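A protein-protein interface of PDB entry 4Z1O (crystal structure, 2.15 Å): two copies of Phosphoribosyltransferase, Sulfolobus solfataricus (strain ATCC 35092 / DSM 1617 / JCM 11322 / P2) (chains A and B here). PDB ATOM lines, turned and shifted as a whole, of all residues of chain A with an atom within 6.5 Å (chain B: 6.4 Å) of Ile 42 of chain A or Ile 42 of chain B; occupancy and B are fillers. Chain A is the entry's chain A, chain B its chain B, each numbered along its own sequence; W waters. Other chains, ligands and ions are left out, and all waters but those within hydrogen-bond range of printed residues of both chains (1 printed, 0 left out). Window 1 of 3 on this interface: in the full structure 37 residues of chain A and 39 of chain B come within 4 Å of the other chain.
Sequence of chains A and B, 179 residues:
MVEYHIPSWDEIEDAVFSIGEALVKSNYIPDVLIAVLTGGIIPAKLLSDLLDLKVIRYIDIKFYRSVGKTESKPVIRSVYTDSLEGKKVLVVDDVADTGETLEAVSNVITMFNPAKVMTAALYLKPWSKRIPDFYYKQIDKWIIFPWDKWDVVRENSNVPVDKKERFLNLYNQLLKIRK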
ATOM      1  N   TRP A   9     -11.027  13.623   1.983  1.00  0.00           N
ATOM      2  CA  TRP A   9     -11.509  13.630   3.375  1.00  0.00           C
ATOM      3  C   TRP A   9     -10.803  12.535   4.163  1.00  0.00           C
ATOM      4  O   TRP A   9     -10.557  12.667   5.373  1.00  0.00           O
ATOM      5  CB  TRP A   9     -13.034  13.420   3.463  1.00  0.00           C
ATOM      6  CG  TRP A   9     -13.857  14.596   3.024  1.00  0.00           C
ATOM      7  CD1 TRP A   9     -14.442  14.774   1.799  1.00  0.00           C
ATOM      8  CD2 TRP A   9     -14.197  15.753   3.801  1.00  0.00           C
ATOM      9  NE1 TRP A   9     -15.107  15.974   1.763  1.00  0.00           N
ATOM     10  CE2 TRP A   9     -14.976  16.593   2.979  1.00  0.00           C
ATOM     11  CE3 TRP A   9     -13.909  16.169   5.103  1.00  0.00           C
ATOM     12  CZ2 TRP A   9     -15.472  17.824   3.424  1.00  0.00           C
ATOM     13  CZ3 TRP A   9     -14.400  17.392   5.539  1.00  0.00           C
ATOM     14  CH2 TRP A   9     -15.171  18.202   4.702  1.00  0.00           C
ATOM     15  N   ILE A  12      -7.696  14.078   5.188  1.00  0.00           N
ATOM     16  CA  ILE A  12      -8.056  15.026   6.235  1.00  0.00           C
ATOM     17  C   ILE A  12      -8.267  14.309   7.561  1.00  0.00           C
ATOM     18  O   ILE A  12      -7.810  14.779   8.605  1.00  0.00           O
ATOM     19  CB  ILE A  12      -9.335  15.807   5.887  1.00  0.00           C
ATOM     20  CG1 ILE A  12      -9.164  16.528   4.548  1.00  0.00           C
ATOM     21  CG2 ILE A  12      -9.699  16.766   7.030  1.00  0.00           C
ATOM     22  CD1 ILE A  12      -8.096  17.615   4.577  1.00  0.00           C
ATOM     23  N   VAL A  16      -6.146  14.549  11.066  1.00  0.00           N
ATOM     24  CA  VAL A  16      -6.794  14.851  12.324  1.00  0.00           C
ATOM     25  C   VAL A  16      -6.399  13.805  13.358  1.00  0.00           C
ATOM     26  O   VAL A  16      -6.074  14.150  14.497  1.00  0.00           O
ATOM     27  CB  VAL A  16      -8.333  14.940  12.141  1.00  0.00           C
ATOM     28  CG1 VAL A  16      -9.066  14.799  13.479  1.00  0.00           C
ATOM     29  CG2 VAL A  16      -8.711  16.257  11.422  1.00  0.00           C
ATOM     30  N   THR A  38     -12.926  30.711   9.307  1.00  0.00           N
ATOM     31  CA  THR A  38     -13.893  29.616   9.192  1.00  0.00           C
ATOM     32  C   THR A  38     -13.200  28.332   8.726  1.00  0.00           C
ATOM     33  O   THR A  38     -13.802  27.265   8.675  1.00  0.00           O
ATOM     34  CB  THR A  38     -15.026  29.959   8.196  1.00  0.00           C
ATOM     35  OG1 THR A  38     -14.464  30.238   6.911  1.00  0.00           O
ATOM     36  CG2 THR A  38     -15.811  31.156   8.661  1.00  0.00           C
ATOM     37  N   GLY A  39     -11.926  28.444   8.371  1.00  0.00           N
ATOM     38  CA  GLY A  39     -11.180  27.308   7.867  1.00  0.00           C
ATOM     39  C   GLY A  39     -10.850  26.268   8.925  1.00  0.00           C
ATOM     40  O   GLY A  39     -10.713  25.090   8.605  1.00  0.00           O
ATOM     41  N   GLY A  40     -10.715  26.697  10.180  1.00  0.00           N
ATOM     42  CA  GLY A  40     -10.380  25.779  11.259  1.00  0.00           C
ATOM     43  C   GLY A  40     -11.618  25.160  11.895  1.00  0.00           C
ATOM     44  O   GLY A  40     -11.540  24.486  12.932  1.00  0.00           O
ATOM     45  N   ILE A  41     -12.765  25.411  11.268  1.00  0.00           N
ATOM     46  CA  ILE A  41     -14.080  24.971  11.748  1.00  0.00           C
ATOM     47  C   ILE A  41     -14.232  23.440  11.696  1.00  0.00           C
ATOM     48  O   ILE A  41     -14.519  22.784  12.705  1.00  0.00           O
ATOM     49  CB  ILE A  41     -15.197  25.701  10.922  1.00  0.00           C
ATOM     50  CG1 ILE A  41     -15.770  26.847  11.729  1.00  0.00           C
ATOM     51  CG2 ILE A  41     -16.286  24.786  10.459  1.00  0.00           C
ATOM     52  CD1 ILE A  41     -16.898  27.605  10.996  1.00  0.00           C
ATOM     53  N   ILE A  42     -13.981  22.872  10.526  1.00  0.00           N
ATOM     54  CA  ILE A  42     -14.081  21.447  10.340  1.00  0.00           C
ATOM     55  C   ILE A  42     -12.942  20.727  11.105  1.00  0.00           C
ATOM     56  O   ILE A  42     -13.221  19.779  11.842  1.00  0.00           O
ATOM     57  CB  ILE A  42     -14.112  21.115   8.836  1.00  0.00           C
ATOM     58  CG1 ILE A  42     -15.412  21.679   8.234  1.00  0.00           C
ATOM     59  CG2 ILE A  42     -13.971  19.633   8.612  1.00  0.00           C
ATOM     60  CD1 ILE A  42     -15.518  21.583   6.741  1.00  0.00           C
ATOM     61  N   PRO A  43     -11.678  21.197  10.984  1.00  0.00           N
ATOM     62  CA  PRO A  43     -10.637  20.618  11.846  1.00  0.00           C
ATOM     63  C   PRO A  43     -10.962  20.628  13.358  1.00  0.00           C
ATOM     64  O   PRO A  43     -10.723  19.627  14.044  1.00  0.00           O
ATOM     65  CB  PRO A  43      -9.422  21.503  11.547  1.00  0.00           C
ATOM     66  CG  PRO A  43      -9.622  21.923  10.147  1.00  0.00           C
ATOM     67  CD  PRO A  43     -11.096  22.136  10.001  1.00  0.00           C
ATOM     68  N   ALA A  44     -11.498  21.726  13.878  1.00  0.00           N
ATOM     69  CA  ALA A  44     -11.817  21.771  15.297  1.00  0.00           C
ATOM     70  C   ALA A  44     -12.901  20.769  15.686  1.00  0.00           C
ATOM     71  O   ALA A  44     -12.869  20.234  16.792  1.00  0.00           O
ATOM     72  CB  ALA A  44     -12.240  23.171  15.704  1.00  0.00           C
ATOM     73  N   LYS A  45     -13.857  20.523  14.792  1.00  0.00           N
ATOM     74  CA  LYS A  45     -14.990  19.664  15.129  1.00  0.00           C
ATOM     75  C   LYS A  45     -14.567  18.217  15.095  1.00  0.00           C
ATOM     76  O   LYS A  45     -15.019  17.417  15.913  1.00  0.00           O
ATOM     77  CB  LYS A  45     -16.177  19.886  14.183  1.00  0.00           C
ATOM     78  CG  LYS A  45     -17.314  18.848  14.323  1.00  0.00           C
ATOM     79  CD  LYS A  45     -17.953  18.828  15.720  1.00  0.00           C
ATOM     80  CE  LYS A  45     -19.140  17.842  15.781  1.00  0.00           C
ATOM     81  NZ  LYS A  45     -19.729  17.715  17.152  1.00  0.00           N
ATOM     82  N   LEU A  46     -13.701  17.892  14.138  1.00  0.00           N
ATOM     83  CA  LEU A  46     -13.178  16.538  14.004  1.00  0.00           C
ATOM     84  C   LEU A  46     -12.241  16.163  15.164  1.00  0.00           C
ATOM     85  O   LEU A  46     -12.309  15.045  15.695  1.00  0.00           O
ATOM     86  CB  LEU A  46     -12.466  16.382  12.662  1.00  0.00           C
ATOM     87  CG  LEU A  46     -13.371  16.526  11.427  1.00  0.00           C
ATOM     88  CD1 LEU A  46     -12.592  16.263  10.121  1.00  0.00           C
ATOM     89  CD2 LEU A  46     -14.594  15.598  11.527  1.00  0.00           C
ATOM     90  N   LEU A  47     -11.369  17.088  15.556  1.00  0.00           N
ATOM     91  CA  LEU A  47     -10.474  16.847  16.689  1.00  0.00           C
ATOM     92  C   LEU A  47     -11.292  16.705  17.968  1.00  0.00           C
ATOM     93  O   LEU A  47     -11.033  15.827  18.790  1.00  0.00           O
ATOM     94  CB  LEU A  47      -9.460  17.976  16.846  1.00  0.00           C
ATOM     95  CG  LEU A  47      -8.365  17.720  17.877  1.00  0.00           C
ATOM     96  CD1 LEU A  47      -7.425  16.588  17.430  1.00  0.00           C
ATOM     97  CD2 LEU A  47      -7.596  18.982  18.135  1.00  0.00           C
ATOM     98  N   VAL A  92      -7.000  25.753  16.974  1.00  0.00           N
ATOM     99  CA  VAL A  92      -7.059  24.884  15.808  1.00  0.00           C
ATOM    100  C   VAL A  92      -7.311  25.656  14.514  1.00  0.00           C
ATOM    101  O   VAL A  92      -8.269  26.436  14.424  1.00  0.00           O
ATOM    102  CB  VAL A  92      -8.164  23.844  15.953  1.00  0.00           C
ATOM    103  CG1 VAL A  92      -8.237  23.008  14.695  1.00  0.00           C
ATOM    104  CG2 VAL A  92      -7.919  22.974  17.187  1.00  0.00           C
ATOM    105  N   PRO A 146     -11.232  20.442   1.120  1.00  0.00           N
ATOM    106  CA  PRO A 146     -12.587  20.110   0.666  1.00  0.00           C
ATOM    107  C   PRO A 146     -13.586  21.235   0.958  1.00  0.00           C
ATOM    108  O   PRO A 146     -14.606  21.316   0.296  1.00  0.00           O
ATOM    109  CB  PRO A 146     -12.926  18.849   1.464  1.00  0.00           C
ATOM    110  CG  PRO A 146     -11.601  18.236   1.802  1.00  0.00           C
ATOM    111  CD  PRO A 146     -10.662  19.408   2.004  1.00  0.00           C
ATOM    112  N   TRP A 147     -13.278  22.090   1.930  1.00  0.00           N
ATOM    113  CA  TRP A 147     -14.174  23.178   2.300  1.00  0.00           C
ATOM    114  C   TRP A 147     -13.818  24.555   1.700  1.00  0.00           C
ATOM    115  O   TRP A 147     -14.456  25.562   2.044  1.00  0.00           O
ATOM    116  CB  TRP A 147     -14.242  23.300   3.828  1.00  0.00           C
ATOM    117  CG  TRP A 147     -12.899  23.371   4.510  1.00  0.00           C
ATOM    118  CD1 TRP A 147     -12.152  24.492   4.743  1.00  0.00           C
ATOM    119  CD2 TRP A 147     -12.154  22.274   5.049  1.00  0.00           C
ATOM    120  NE1 TRP A 147     -10.983  24.159   5.386  1.00  0.00           N
ATOM    121  CE2 TRP A 147     -10.963  22.807   5.584  1.00  0.00           C
ATOM    122  CE3 TRP A 147     -12.376  20.893   5.120  1.00  0.00           C
ATOM    123  CZ2 TRP A 147     -10.005  22.000   6.195  1.00  0.00           C
ATOM    124  CZ3 TRP A 147     -11.418  20.105   5.720  1.00  0.00           C
ATOM    125  CH2 TRP A 147     -10.251  20.659   6.251  1.00  0.00           C
ATOM    126  N   TRP B   9     -18.438  10.736   3.592  1.00  0.00           N
ATOM    127  CA  TRP B   9     -18.175  12.131   3.302  1.00  0.00           C
ATOM    128  C   TRP B   9     -18.720  12.479   1.925  1.00  0.00           C
ATOM    129  O   TRP B   9     -19.158  13.611   1.699  1.00  0.00           O
ATOM    130  CB  TRP B   9     -16.676  12.429   3.368  1.00  0.00           C
ATOM    131  CG  TRP B   9     -16.158  12.642   4.759  1.00  0.00           C
ATOM    132  CD1 TRP B   9     -15.361  11.799   5.471  1.00  0.00           C
ATOM    133  CD2 TRP B   9     -16.412  13.773   5.609  1.00  0.00           C
ATOM    134  NE1 TRP B   9     -15.086  12.333   6.707  1.00  0.00           N
ATOM    135  CE2 TRP B   9     -15.710  13.537   6.815  1.00  0.00           C
ATOM    136  CE3 TRP B   9     -17.140  14.949   5.462  1.00  0.00           C
ATOM    137  CZ2 TRP B   9     -15.736  14.458   7.874  1.00  0.00           C
ATOM    138  CZ3 TRP B   9     -17.165  15.854   6.519  1.00  0.00           C
ATOM    139  CH2 TRP B   9     -16.470  15.601   7.710  1.00  0.00           C
ATOM    140  N   ILE B  12     -22.273  13.330   2.297  1.00  0.00           N
ATOM    141  CA  ILE B  12     -22.473  14.612   2.946  1.00  0.00           C
ATOM    142  C   ILE B  12     -22.316  15.736   1.897  1.00  0.00           C
ATOM    143  O   ILE B  12     -23.127  16.653   1.855  1.00  0.00           O
ATOM    144  CB  ILE B  12     -21.491  14.820   4.123  1.00  0.00           C
ATOM    145  CG1 ILE B  12     -21.737  13.776   5.222  1.00  0.00           C
ATOM    146  CG2 ILE B  12     -21.640  16.227   4.710  1.00  0.00           C
ATOM    147  CD1 ILE B  12     -23.146  13.846   5.864  1.00  0.00           C
ATOM    148  N   VAL B  16     -25.100  18.402   0.984  1.00  0.00           N
ATOM    149  CA  VAL B  16     -24.840  19.831   0.894  1.00  0.00           C
ATOM    150  C   VAL B  16     -25.209  20.355  -0.495  1.00  0.00           C
ATOM    151  O   VAL B  16     -25.901  21.366  -0.612  1.00  0.00           O
ATOM    152  CB  VAL B  16     -23.350  20.142   1.213  1.00  0.00           C
ATOM    153  CG1 VAL B  16     -23.017  21.571   0.866  1.00  0.00           C
ATOM    154  CG2 VAL B  16     -23.043  19.846   2.694  1.00  0.00           C
ATOM    155  N   THR B  38     -23.152  21.797  17.705  1.00  0.00           N
ATOM    156  CA  THR B  38     -21.933  21.683  16.903  1.00  0.00           C
ATOM    157  C   THR B  38     -22.083  20.825  15.642  1.00  0.00           C
ATOM    158  O   THR B  38     -21.201  20.847  14.776  1.00  0.00           O
ATOM    159  CB  THR B  38     -20.764  21.071  17.718  1.00  0.00           C
ATOM    160  OG1 THR B  38     -21.123  19.757  18.183  1.00  0.00           O
ATOM    161  CG2 THR B  38     -20.387  21.963  18.897  1.00  0.00           C
ATOM    162  N   GLY B  39     -23.164  20.048  15.551  1.00  0.00           N
ATOM    163  CA  GLY B  39     -23.377  19.176  14.402  1.00  0.00           C
ATOM    164  C   GLY B  39     -23.621  19.923  13.085  1.00  0.00           C
ATOM    165  O   GLY B  39     -23.384  19.391  11.991  1.00  0.00           O
ATOM    166  N   GLY B  40     -24.091  21.161  13.185  1.00  0.00           N
ATOM    167  CA  GLY B  40     -24.391  21.966  12.005  1.00  0.00           C
ATOM    168  C   GLY B  40     -23.164  22.686  11.464  1.00  0.00           C
ATOM    169  O   GLY B  40     -23.222  23.311  10.404  1.00  0.00           O
ATOM    170  N   ILE B  41     -22.061  22.587  12.206  1.00  0.00           N
ATOM    171  CA  ILE B  41     -20.786  23.239  11.888  1.00  0.00           C
ATOM    172  C   ILE B  41     -20.275  22.887  10.497  1.00  0.00           C
ATOM    173  O   ILE B  41     -20.040  23.769   9.662  1.00  0.00           O
ATOM    174  CB  ILE B  41     -19.691  22.852  12.932  1.00  0.00           C
ATOM    175  CG1 ILE B  41     -19.767  23.728  14.174  1.00  0.00           C
ATOM    176  CG2 ILE B  41     -18.284  22.945  12.365  1.00  0.00           C
ATOM    177  CD1 ILE B  41     -18.886  23.205  15.332  1.00  0.00           C
ATOM    178  N   ILE B  42     -20.095  21.594  10.251  1.00  0.00           N
ATOM    179  CA  ILE B  42     -19.544  21.156   8.980  1.00  0.00           C
ATOM    180  C   ILE B  42     -20.550  21.432   7.839  1.00  0.00           C
ATOM    181  O   ILE B  42     -20.158  22.036   6.837  1.00  0.00           O
ATOM    182  CB  ILE B  42     -19.109  19.671   9.055  1.00  0.00           C
ATOM    183  CG1 ILE B  42     -18.042  19.509  10.161  1.00  0.00           C
ATOM    184  CG2 ILE B  42     -18.653  19.146   7.691  1.00  0.00           C
ATOM    185  CD1 ILE B  42     -17.229  18.223  10.087  1.00  0.00           C
ATOM    186  N   PRO B  43     -21.844  21.045   7.999  1.00  0.00           N
ATOM    187  CA  PRO B  43     -22.836  21.447   6.992  1.00  0.00           C
ATOM    188  C   PRO B  43     -22.811  22.946   6.616  1.00  0.00           C
ATOM    189  O   PRO B  43     -22.794  23.266   5.427  1.00  0.00           O
ATOM    190  CB  PRO B  43     -24.169  21.087   7.665  1.00  0.00           C
ATOM    191  CG  PRO B  43     -23.842  19.886   8.472  1.00  0.00           C
ATOM    192  CD  PRO B  43     -22.449  20.155   9.011  1.00  0.00           C
ATOM    193  N   ALA B  44     -22.800  23.830   7.610  1.00  0.00           N
ATOM    194  CA  ALA B  44     -22.800  25.277   7.371  1.00  0.00           C
ATOM    195  C   ALA B  44     -21.557  25.767   6.621  1.00  0.00           C
ATOM    196  O   ALA B  44     -21.655  26.626   5.744  1.00  0.00           O
ATOM    197  CB  ALA B  44     -22.926  26.020   8.666  1.00  0.00           C
ATOM    198  N   LYS B  45     -20.391  25.229   6.972  1.00  0.00           N
ATOM    199  CA  LYS B  45     -19.159  25.643   6.319  1.00  0.00           C
ATOM    200  C   LYS B  45     -19.179  25.201   4.853  1.00  0.00           C
ATOM    201  O   LYS B  45     -18.845  25.977   3.959  1.00  0.00           O
ATOM    202  CB  LYS B  45     -17.929  25.078   7.051  1.00  0.00           C
ATOM    203  CG  LYS B  45     -16.600  25.315   6.331  1.00  0.00           C
ATOM    204  CD  LYS B  45     -16.324  26.799   6.067  1.00  0.00           C
ATOM    205  CE  LYS B  45     -14.977  26.989   5.366  1.00  0.00           C
ATOM    206  NZ  LYS B  45     -14.671  28.435   5.025  1.00  0.00           N
ATOM    207  N   LEU B  46     -19.599  23.964   4.603  1.00  0.00           N
ATOM    208  CA  LEU B  46     -19.568  23.465   3.240  1.00  0.00           C
ATOM    209  C   LEU B  46     -20.560  24.249   2.356  1.00  0.00           C
ATOM    210  O   LEU B  46     -20.307  24.464   1.172  1.00  0.00           O
ATOM    211  CB  LEU B  46     -19.865  21.964   3.198  1.00  0.00           C
ATOM    212  CG  LEU B  46     -18.804  21.032   3.801  1.00  0.00           C
ATOM    213  CD1 LEU B  46     -19.178  19.560   3.594  1.00  0.00           C
ATOM    214  CD2 LEU B  46     -17.410  21.317   3.240  1.00  0.00           C
ATOM    215  N   LEU B  47     -21.679  24.670   2.935  1.00  0.00           N
ATOM    216  CA  LEU B  47     -22.716  25.358   2.161  1.00  0.00           C
ATOM    217  C   LEU B  47     -22.250  26.766   1.876  1.00  0.00           C
ATOM    218  O   LEU B  47     -22.515  27.320   0.816  1.00  0.00           O
ATOM    219  CB  LEU B  47     -24.053  25.378   2.906  1.00  0.00           C
ATOM    220  CG  LEU B  47     -25.280  25.892   2.149  1.00  0.00           C
ATOM    221  CD1 LEU B  47     -25.597  25.060   0.881  1.00  0.00           C
ATOM    222  CD2 LEU B  47     -26.491  25.953   3.077  1.00  0.00           C
ATOM    223  N   PRO B 146     -19.987  11.663   9.906  1.00  0.00           N
ATOM    224  CA  PRO B 146     -18.528  11.660   9.977  1.00  0.00           C
ATOM    225  C   PRO B 146     -17.949  12.440  11.163  1.00  0.00           C
ATOM    226  O   PRO B 146     -16.878  12.059  11.638  1.00  0.00           O
ATOM    227  CB  PRO B 146     -18.125  12.309   8.652  1.00  0.00           C
ATOM    228  CG  PRO B 146     -19.209  11.918   7.701  1.00  0.00           C
ATOM    229  CD  PRO B 146     -20.473  11.972   8.545  1.00  0.00           C
ATOM    230  N   TRP B 147     -18.633  13.482  11.638  1.00  0.00           N
ATOM    231  CA  TRP B 147     -18.113  14.311  12.726  1.00  0.00           C
ATOM    232  C   TRP B 147     -18.581  13.932  14.137  1.00  0.00           C
ATOM    233  O   TRP B 147     -18.201  14.593  15.116  1.00  0.00           O
ATOM    234  CB  TRP B 147     -18.469  15.780  12.467  1.00  0.00           C
ATOM    235  CG  TRP B 147     -19.893  15.983  12.096  1.00  0.00           C
ATOM    236  CD1 TRP B 147     -20.938  16.165  12.948  1.00  0.00           C
ATOM    237  CD2 TRP B 147     -20.437  16.022  10.775  1.00  0.00           C
ATOM    238  NE1 TRP B 147     -22.106  16.309  12.240  1.00  0.00           N
ATOM    239  CE2 TRP B 147     -21.824  16.226  10.888  1.00  0.00           C
ATOM    240  CE3 TRP B 147     -19.887  15.903   9.486  1.00  0.00           C
ATOM    241  CZ2 TRP B 147     -22.670  16.327   9.793  1.00  0.00           C
ATOM    242  CZ3 TRP B 147     -20.721  16.002   8.388  1.00  0.00           C
ATOM    243  CH2 TRP B 147     -22.103  16.209   8.546  1.00  0.00           C
HETATM  244  O   HOH W   1     -21.692  16.782  19.866  1.00  0.00           O
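Water W1 lies within hydrogen-bond range of OG1 of Thr 38 of chain B (3.5 Å) and NZ of Lys 45 of chain A (3.5 Å).
OG1 of Thr 38 of chain A is in hydrogen-bond range of NZ of Lys 45 of chain B (2.6 Å). NZ of Lys 45 of chain A sits at hydrogen-bond distance from OG1 of Thr 38 of chain B, 2.7 Å away.
Hydrophobic or aromatic side chains of chain A within 4 Å of the printed part of chain B: Trp 9, Ile 41, Ile 42, Leu 46 and Trp 147. Hydrophobic or aromatic side chains of chain B within 4 Å of the printed part of chain A: Trp 9, Ile 41, Ile 42, Leu 46 and Trp 147. Among the printed residues, no Asp or Glu carboxylate lies within 4 Å of a Lys or Arg side-chain nitrogen of the other chain.
Printed residues of chain B within 4 Å of Thr 38 of chain A: Lys 45 (2.6 Å). Of the printed residues of chain B, Ile 41 of chain A touches Ile 41 (3.3 Å) and Lys 45 (3.8 Å). Printed residues of chain A within 4 Å of Ile 41 of chain B: Ile 41. Of the printed residues of chain A, Ile 42 of chain B touches Ile 42 (3.8 Å) and Leu 46 (3.99 Å).
Among the printed residues, merely in contact across the chains: Trp 9 of chain A with Trp 9 of chain B (3.3 Å), Trp 9 of chain A with Leu 46 of chain B (3.999 Å), Ile 41 of chain A with Ile 41 of chain B (3.3 Å), Ile 41 of chain A with Lys 45 of chain B (3.8 Å), Ile 42 of chain A with Ile 42 of chain B (3.8 Å), Ile 42 of chain A with Lys 45 of chain B (3.9 Å), Ile 42 of chain A with Leu 46 of chain B (3.99 Å), Lys 45 of chain A with Trp 147 of chain B (3.4 Å), Leu 46 of chain A with Trp 9 of chain B (3.99 Å), Leu 46 of chain A with Ile 42 of chain B (3.99 Å), Leu 46 of chain A with Trp 147 of chain B (3.9 Å), Trp 147 of chain A with Lys 45 of chain B (3.7 Å) and Trp 147 of chain A with Leu 46 of chain B (3.8 Å).
The backbone carbonyl oxygen (O) of Gly 39 of chain B is in hydrogen-bond range of the indole nitrogen (NE1) of Trp 147 of chain B. The backbone carbonyl oxygen (O) of Gly 39 of chain A sits at hydrogen-bond distance from the indole nitrogen (NE1) of Trp 147 of chain A, at 3.4 Å.
Trp 9 of chain A touches its own counterpart, Trp 9 of chain B. Ile 42 of chain A touches Leu 46 of chain B, and with the chains exchanged Leu 46 of chain A touches Ile 42 of chain B. Lys 45 of chain A touches Trp 147 of chain B, and with the chains exchanged Trp 147 of chain A touches Lys 45 of chain B. Leu 46 of chain A touches Trp 147 of chain B, and with the chains exchanged Trp 147 of chain A touches Leu 46 of chain B.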
